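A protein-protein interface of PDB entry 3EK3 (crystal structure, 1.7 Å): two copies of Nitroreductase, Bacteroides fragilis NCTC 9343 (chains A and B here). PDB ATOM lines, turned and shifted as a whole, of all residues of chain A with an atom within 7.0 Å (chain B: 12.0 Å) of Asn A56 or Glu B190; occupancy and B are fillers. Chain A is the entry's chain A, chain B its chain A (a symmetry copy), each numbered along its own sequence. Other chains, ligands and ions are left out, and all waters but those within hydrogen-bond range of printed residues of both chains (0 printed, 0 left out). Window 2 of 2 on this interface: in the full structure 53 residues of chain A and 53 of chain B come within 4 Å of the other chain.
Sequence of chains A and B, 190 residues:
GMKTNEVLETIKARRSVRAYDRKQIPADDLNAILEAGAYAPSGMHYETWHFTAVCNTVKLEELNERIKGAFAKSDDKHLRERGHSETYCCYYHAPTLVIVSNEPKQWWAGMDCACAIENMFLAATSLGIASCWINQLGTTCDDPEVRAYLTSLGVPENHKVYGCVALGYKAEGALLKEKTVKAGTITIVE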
ATOM      1  N   GLN A  24      13.209  10.522 -24.771  1.00  0.00           N
ATOM      2  CA  GLN A  24      12.501   9.264 -24.841  1.00  0.00           C
ATOM      3  C   GLN A  24      12.505   8.747 -26.263  1.00  0.00           C
ATOM      4  O   GLN A  24      12.565   9.524 -27.216  1.00  0.00           O
ATOM      5  CB  GLN A  24      11.082   9.432 -24.304  1.00  0.00           C
ATOM      6  CG  GLN A  24      10.241   8.199 -24.246  1.00  0.00           C
ATOM      7  CD  GLN A  24      10.834   7.147 -23.361  1.00  0.00           C
ATOM      8  OE1 GLN A  24      11.721   6.414 -23.776  1.00  0.00           O
ATOM      9  NE2 GLN A  24      10.381   7.090 -22.114  1.00  0.00           N
ATOM     10  N   ALA A  53       7.262  -2.697 -20.130  1.00  0.00           N
ATOM     11  CA  ALA A  53       8.045  -1.565 -20.575  1.00  0.00           C
ATOM     12  C   ALA A  53       7.691  -0.348 -19.733  1.00  0.00           C
ATOM     13  O   ALA A  53       6.587   0.175 -19.817  1.00  0.00           O
ATOM     14  CB  ALA A  53       7.816  -1.284 -22.068  1.00  0.00           C
ATOM     15  N   VAL A  54       8.628   0.098 -18.906  1.00  0.00           N
ATOM     16  CA  VAL A  54       8.406   1.236 -18.040  1.00  0.00           C
ATOM     17  C   VAL A  54       9.094   2.459 -18.642  1.00  0.00           C
ATOM     18  O   VAL A  54      10.316   2.494 -18.738  1.00  0.00           O
ATOM     19  CB  VAL A  54       8.937   0.993 -16.618  1.00  0.00           C
ATOM     20  CG1 VAL A  54       8.618   2.200 -15.686  1.00  0.00           C
ATOM     21  CG2 VAL A  54       8.339  -0.291 -16.056  1.00  0.00           C
ATOM     22  N   CYS A  55       8.284   3.448 -19.030  1.00  0.00           N
ATOM     23  CA  CYS A  55       8.742   4.625 -19.739  1.00  0.00           C
ATOM     24  C   CYS A  55       8.630   5.899 -18.912  1.00  0.00           C
ATOM     25  O   CYS A  55       8.806   6.977 -19.420  1.00  0.00           O
ATOM     26  CB  CYS A  55       7.900   4.777 -20.985  1.00  0.00           C
ATOM     27  SG  CYS A  55       7.978   3.352 -22.066  1.00  0.00           S
ATOM     28  N   ASN A  56       8.363   5.758 -17.628  1.00  0.00           N
ATOM     29  CA  ASN A  56       8.052   6.898 -16.793  1.00  0.00           C
ATOM     30  C   ASN A  56       9.226   7.129 -15.839  1.00  0.00           C
ATOM     31  O   ASN A  56       9.564   6.270 -15.037  1.00  0.00           O
ATOM     32  CB  ASN A  56       6.767   6.564 -16.038  1.00  0.00           C
ATOM     33  CG  ASN A  56       6.240   7.717 -15.237  1.00  0.00           C
ATOM     34  OD1 ASN A  56       6.896   8.200 -14.330  1.00  0.00           O
ATOM     35  ND2 ASN A  56       5.048   8.174 -15.583  1.00  0.00           N
ATOM     36  N   THR A  57       9.862   8.285 -15.949  1.00  0.00           N
ATOM     37  CA  THR A  57      11.060   8.577 -15.169  1.00  0.00           C
ATOM     38  C   THR A  57      10.826   8.514 -13.689  1.00  0.00           C
ATOM     39  O   THR A  57      11.664   7.958 -12.976  1.00  0.00           O
ATOM     40  CB  THR A  57      11.647   9.928 -15.560  1.00  0.00           C
ATOM     41  OG1 THR A  57      12.083   9.836 -16.919  1.00  0.00           O
ATOM     42  CG2 THR A  57      12.846  10.288 -14.702  1.00  0.00           C
ATOM     43  N   VAL A  58       9.679   9.011 -13.220  1.00  0.00           N
ATOM     44  CA  VAL A  58       9.369   8.967 -11.781  1.00  0.00           C
ATOM     45  C   VAL A  58       9.310   7.536 -11.292  1.00  0.00           C
ATOM     46  O   VAL A  58       9.876   7.206 -10.258  1.00  0.00           O
ATOM     47  CB  VAL A  58       8.030   9.670 -11.423  1.00  0.00           C
ATOM     48  CG1 VAL A  58       7.685   9.427  -9.960  1.00  0.00           C
ATOM     49  CG2 VAL A  58       8.098  11.151 -11.701  1.00  0.00           C
ATOM     50  N   LYS A  59       8.608   6.676 -12.014  1.00  0.00           N
ATOM     51  CA  LYS A  59       8.480   5.278 -11.580  1.00  0.00           C
ATOM     52  C   LYS A  59       9.822   4.546 -11.657  1.00  0.00           C
ATOM     53  O   LYS A  59      10.130   3.712 -10.812  1.00  0.00           O
ATOM     54  CB  LYS A  59       7.440   4.542 -12.415  1.00  0.00           C
ATOM     55  CG  LYS A  59       6.058   5.153 -12.359  1.00  0.00           C
ATOM     56  CD  LYS A  59       5.070   4.313 -13.149  1.00  0.00           C
ATOM     57  CE  LYS A  59       3.816   5.096 -13.543  1.00  0.00           C
ATOM     58  NZ  LYS A  59       2.993   5.744 -12.480  1.00  0.00           N
ATOM     59  N   LEU A  60      10.623   4.851 -12.666  1.00  0.00           N
ATOM     60  CA  LEU A  60      11.955   4.219 -12.750  1.00  0.00           C
ATOM     61  C   LEU A  60      12.815   4.570 -11.524  1.00  0.00           C
ATOM     62  O   LEU A  60      13.461   3.721 -10.951  1.00  0.00           O
ATOM     63  CB  LEU A  60      12.647   4.604 -14.033  1.00  0.00           C
ATOM     64  CG  LEU A  60      12.037   3.959 -15.258  1.00  0.00           C
ATOM     65  CD1 LEU A  60      12.611   4.669 -16.526  1.00  0.00           C
ATOM     66  CD2 LEU A  60      12.192   2.420 -15.258  1.00  0.00           C
ATOM     67  N   GLU A  61      12.777   5.838 -11.133  1.00  0.00           N
ATOM     68  CA  GLU A  61      13.518   6.295  -9.982  1.00  0.00           C
ATOM     69  C   GLU A  61      13.028   5.625  -8.706  1.00  0.00           C
ATOM     70  O   GLU A  61      13.821   5.201  -7.878  1.00  0.00           O
ATOM     71  CB  GLU A  61      13.468   7.828  -9.909  1.00  0.00           C
ATOM     72  CG  GLU A  61      14.195   8.468 -11.092  1.00  0.00           C
ATOM     73  CD  GLU A  61      14.349   9.980 -10.985  1.00  0.00           C
ATOM     74  OE1 GLU A  61      13.739  10.594 -10.065  1.00  0.00           O
ATOM     75  OE2 GLU A  61      15.092  10.543 -11.839  1.00  0.00           O
ATOM     76  N   GLU A  62      11.711   5.501  -8.541  1.00  0.00           N
ATOM     77  CA  GLU A  62      11.156   4.825  -7.377  1.00  0.00           C
ATOM     78  C   GLU A  62      11.574   3.342  -7.298  1.00  0.00           C
ATOM     79  O   GLU A  62      11.883   2.825  -6.219  1.00  0.00           O
ATOM     80  CB  GLU A  62       9.615   4.947  -7.367  1.00  0.00           C
ATOM     81  CG  GLU A  62       9.116   6.352  -7.070  1.00  0.00           C
ATOM     82  CD  GLU A  62       7.600   6.448  -6.896  1.00  0.00           C
ATOM     83  OE1 GLU A  62       6.863   5.585  -7.423  1.00  0.00           O
ATOM     84  OE2 GLU A  62       7.158   7.357  -6.146  1.00  0.00           O
ATOM     85  N   TYR A  91      19.877   1.481 -13.958  1.00  0.00           N
ATOM     86  CA  TYR A  91      19.516   1.564 -15.380  1.00  0.00           C
ATOM     87  C   TYR A  91      20.129   2.771 -16.083  1.00  0.00           C
ATOM     88  O   TYR A  91      19.775   3.107 -17.216  1.00  0.00           O
ATOM     89  CB  TYR A  91      17.976   1.516 -15.592  1.00  0.00           C
ATOM     90  CG  TYR A  91      17.261   2.666 -14.947  1.00  0.00           C
ATOM     91  CD1 TYR A  91      16.919   2.622 -13.617  1.00  0.00           C
ATOM     92  CD2 TYR A  91      17.001   3.827 -15.633  1.00  0.00           C
ATOM     93  CE1 TYR A  91      16.330   3.679 -12.998  1.00  0.00           C
ATOM     94  CE2 TYR A  91      16.404   4.891 -15.022  1.00  0.00           C
ATOM     95  CZ  TYR A  91      16.065   4.817 -13.691  1.00  0.00           C
ATOM     96  OH  TYR A  91      15.480   5.882 -13.015  1.00  0.00           O
ATOM     97  N   PRO A  95      15.738   6.397 -20.503  1.00  0.00           N
ATOM     98  CA  PRO A  95      14.332   6.829 -20.399  1.00  0.00           C
ATOM     99  C   PRO A  95      13.286   5.703 -20.355  1.00  0.00           C
ATOM    100  O   PRO A  95      12.126   5.941 -19.965  1.00  0.00           O
ATOM    101  CB  PRO A  95      14.172   7.691 -21.659  1.00  0.00           C
ATOM    102  CG  PRO A  95      15.082   7.104 -22.608  1.00  0.00           C
ATOM    103  CD  PRO A  95      16.297   6.727 -21.817  1.00  0.00           C
ATOM    104  N   THR A  96      13.698   4.494 -20.746  1.00  0.00           N
ATOM    105  CA  THR A  96      12.847   3.289 -20.800  1.00  0.00           C
ATOM    106  C   THR A  96      13.623   2.089 -20.246  1.00  0.00           C
ATOM    107  O   THR A  96      14.804   1.907 -20.537  1.00  0.00           O
ATOM    108  CB  THR A  96      12.323   3.001 -22.231  1.00  0.00           C
ATOM    109  OG1 THR A  96      11.366   4.003 -22.582  1.00  0.00           O
ATOM    110  CG2 THR A  96      11.632   1.612 -22.340  1.00  0.00           C
ATOM    111  N   LEU A  97      12.955   1.323 -19.393  1.00  0.00           N
ATOM    112  CA  LEU A  97      13.439   0.028 -18.958  1.00  0.00           C
ATOM    113  C   LEU A  97      12.366  -1.024 -19.193  1.00  0.00           C
ATOM    114  O   LEU A  97      11.246  -0.883 -18.705  1.00  0.00           O
ATOM    115  CB  LEU A  97      13.762   0.074 -17.481  1.00  0.00           C
ATOM    116  CG  LEU A  97      14.408  -1.154 -16.870  1.00  0.00           C
ATOM    117  CD1 LEU A  97      15.839  -1.343 -17.360  1.00  0.00           C
ATOM    118  CD2 LEU A  97      14.382  -1.003 -15.378  1.00  0.00           C
ATOM    119  N   TYR A 149       6.354  -3.074  -5.680  1.00  0.00           N
ATOM    120  CA  TYR A 149       6.529  -2.115  -6.779  1.00  0.00           C
ATOM    121  C   TYR A 149       6.317  -2.785  -8.132  1.00  0.00           C
ATOM    122  O   TYR A 149       5.569  -2.287  -8.966  1.00  0.00           O
ATOM    123  CB  TYR A 149       7.902  -1.390  -6.703  1.00  0.00           C
ATOM    124  CG  TYR A 149       7.793  -0.022  -7.303  1.00  0.00           C
ATOM    125  CD1 TYR A 149       7.871   0.140  -8.687  1.00  0.00           C
ATOM    126  CD2 TYR A 149       7.478   1.098  -6.517  1.00  0.00           C
ATOM    127  CE1 TYR A 149       7.695   1.366  -9.275  1.00  0.00           C
ATOM    128  CE2 TYR A 149       7.286   2.371  -7.108  1.00  0.00           C
ATOM    129  CZ  TYR A 149       7.377   2.489  -8.482  1.00  0.00           C
ATOM    130  OH  TYR A 149       7.182   3.689  -9.120  1.00  0.00           O
ATOM    131  N   LEU A 153       3.428  -2.186 -11.117  1.00  0.00           N
ATOM    132  CA  LEU A 153       3.772  -1.914 -12.524  1.00  0.00           C
ATOM    133  C   LEU A 153       3.122  -2.905 -13.483  1.00  0.00           C
ATOM    134  O   LEU A 153       3.081  -2.677 -14.679  1.00  0.00           O
ATOM    135  CB  LEU A 153       5.291  -1.955 -12.711  1.00  0.00           C
ATOM    136  CG  LEU A 153       6.052  -0.810 -12.059  1.00  0.00           C
ATOM    137  CD1 LEU A 153       7.532  -1.201 -12.083  1.00  0.00           C
ATOM    138  CD2 LEU A 153       5.779   0.534 -12.795  1.00  0.00           C
ATOM    139  N   ILE B 186       2.764  -8.091 -23.511  1.00  0.00           N
ATOM    140  CA  ILE B 186       3.346  -6.747 -23.356  1.00  0.00           C
ATOM    141  C   ILE B 186       2.457  -5.829 -22.508  1.00  0.00           C
ATOM    142  O   ILE B 186       1.239  -5.749 -22.719  1.00  0.00           O
ATOM    143  CB  ILE B 186       3.595  -6.098 -24.731  1.00  0.00           C
ATOM    144  CG1 ILE B 186       4.620  -6.910 -25.524  1.00  0.00           C
ATOM    145  CG2 ILE B 186       4.044  -4.611 -24.557  1.00  0.00           C
ATOM    146  CD1 ILE B 186       4.635  -6.607 -27.008  1.00  0.00           C
ATOM    147  N   THR B 187       3.081  -5.159 -21.536  1.00  0.00           N
ATOM    148  CA  THR B 187       2.476  -4.079 -20.750  1.00  0.00           C
ATOM    149  C   THR B 187       3.388  -2.851 -20.970  1.00  0.00           C
ATOM    150  O   THR B 187       4.616  -2.963 -20.859  1.00  0.00           O
ATOM    151  CB  THR B 187       2.408  -4.443 -19.238  1.00  0.00           C
ATOM    152  OG1 THR B 187       1.480  -5.497 -19.043  1.00  0.00           O
ATOM    153  CG2 THR B 187       1.984  -3.232 -18.326  1.00  0.00           C
ATOM    154  N   ILE B 188       2.795  -1.713 -21.322  1.00  0.00           N
ATOM    155  CA  ILE B 188       3.525  -0.457 -21.392  1.00  0.00           C
ATOM    156  C   ILE B 188       2.995   0.491 -20.323  1.00  0.00           C
ATOM    157  O   ILE B 188       1.787   0.687 -20.169  1.00  0.00           O
ATOM    158  CB  ILE B 188       3.443   0.163 -22.784  1.00  0.00           C
ATOM    159  CG1 ILE B 188       4.125  -0.744 -23.818  1.00  0.00           C
ATOM    160  CG2 ILE B 188       4.127   1.532 -22.805  1.00  0.00           C
ATOM    161  CD1 ILE B 188       3.877  -0.303 -25.235  1.00  0.00           C
ATOM    162  N   VAL B 189       3.924   1.027 -19.543  1.00  0.00           N
ATOM    163  CA  VAL B 189       3.607   1.928 -18.466  1.00  0.00           C
ATOM    164  C   VAL B 189       4.196   3.264 -18.848  1.00  0.00           C
ATOM    165  O   VAL B 189       5.423   3.434 -18.817  1.00  0.00           O
ATOM    166  CB  VAL B 189       4.241   1.485 -17.158  1.00  0.00           C
ATOM    167  CG1 VAL B 189       3.881   2.462 -16.042  1.00  0.00           C
ATOM    168  CG2 VAL B 189       3.814   0.094 -16.789  1.00  0.00           C
ATOM    169  N   GLU B 190       3.317   4.202 -19.184  1.00  0.00           N
ATOM    170  CA  GLU B 190       3.737   5.446 -19.805  1.00  0.00           C
ATOM    171  C   GLU B 190       4.307   6.412 -18.788  1.00  0.00           C
ATOM    172  O   GLU B 190       3.786   6.503 -17.682  1.00  0.00           O
ATOM    173  CB  GLU B 190       2.560   6.105 -20.502  1.00  0.00           C
ATOM    174  CG  GLU B 190       2.070   5.301 -21.674  1.00  0.00           C
ATOM    175  CD  GLU B 190       1.072   6.072 -22.520  1.00  0.00           C
ATOM    176  OE1 GLU B 190       0.311   6.884 -21.960  1.00  0.00           O
ATOM    177  OE2 GLU B 190       1.052   5.850 -23.748  1.00  0.00           O
ATOM    178  OXT GLU B 190       5.278   7.115 -19.108  1.00  0.00           O
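Asn A56 touches two residues of chain B. Glu B190 touches two residues of chain A. Of the printed residues of chain B, Cys A55 touches Val B189 and Glu B190. No residue of chain B comes within 4 Å of Thr A57. Of chain B, only Val B189 comes within 4 Å of Lys A59. No residue of chain B comes within 4 Å of Leu A60. Printed residues of chain A within 4 Å of Val B189: Ala A53, Val A54, Cys A55, Asn A56, Lys A59 and Leu A153. Printed residues of chain A within 4 Å of Ile B188: Ala A53 (3.5 Å). Of the printed residues of chain B, Leu A153 touches Thr B187 and Val B189. Thr A96 touches none of the printed residues of chain B. Glu A62 touches none of the printed residues of chain B. The nearest residue of chain B that does not touch Asn A56 is Ile B188 (7.9 Å). The nearest printed residue of chain B that does not touch Ala A53 is Glu B190 (5.2 Å).
The backbone carbonyl oxygen (O) of Thr B187 lies within hydrogen-bond range of the backbone NH (N) of Ala A53 (2.8 Å). N of Val B189 sits at hydrogen-bond distance from O of Ala A53 (2.8 Å). The backbone NH of Cys A55 lies within hydrogen-bond range of the backbone carbonyl oxygen of Val B189 (2.9 Å). ND2 of Asn A56 is in hydrogen-bond range of O of Glu B190, at 3.0 Å.
Printed residues of chain B that touch a printed residue of chain A: Thr B187, Ile B188, Val B189 and Glu B190. Of the 17 printed residues of chain A, 6 touch a printed residue of chain B. Printed residues of chain A that touch a printed residue of chain B: Ala A53, Val A54, Cys A55, Asn A56, Lys A59 and Leu A153. Hydrophobic or aromatic side chains of chain A within 4 Å of the printed part of chain B: Ala A53. Among the printed residues, no Asp or Glu carboxylate lies within 4 Å of a Lys or Arg side-chain nitrogen of the other chain.
The side-chain amide nitrogen of Gln A24 sits at hydrogen-bond distance from the backbone carbonyl oxygen of Cys A55, 3.1 Å away. The backbone NH (N) of Val A54 lies within hydrogen-bond range of the backbone carbonyl oxygen (O) of Leu A97 (2.8 Å). SG of Cys A55 lies within hydrogen-bond range of OG1 of Thr A96 (3.5 Å). The backbone NH (N) of Val A58 sits at hydrogen-bond distance from the side-chain amide oxygen (OD1) of Asn A56 (3.1 Å). The side-chain amide oxygen (OD1) of Asn A56 is in hydrogen-bond range of the backbone NH (N) of Lys A59 (3.3 Å). The side-chain hydroxyl (OH) of Tyr A149 lies close to the backbone carbonyl oxygen (O) of Lys A59 (3.4 Å).
No position is printed for both chains. Of the 11 pairs that touch across the chains among the printed residues, none has its exchanged pair printed and touching as well.
CA of Ile B188 touches O of Ala A53, 3.5 Å away. O of Val B189 touches CA of Val A54 (3.8 Å). Glu B190 touches Cys A55. N of Asn A56 touches O of Val B189, 3.9 Å away. CG1 of Val B189 touches CE of Lys A59 (3.6 Å). Leu A153 touches Thr B187 (O to CG2, 3.8 Å). Val B189 touches Leu A153 (CG2 to O, 3.6 Å).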
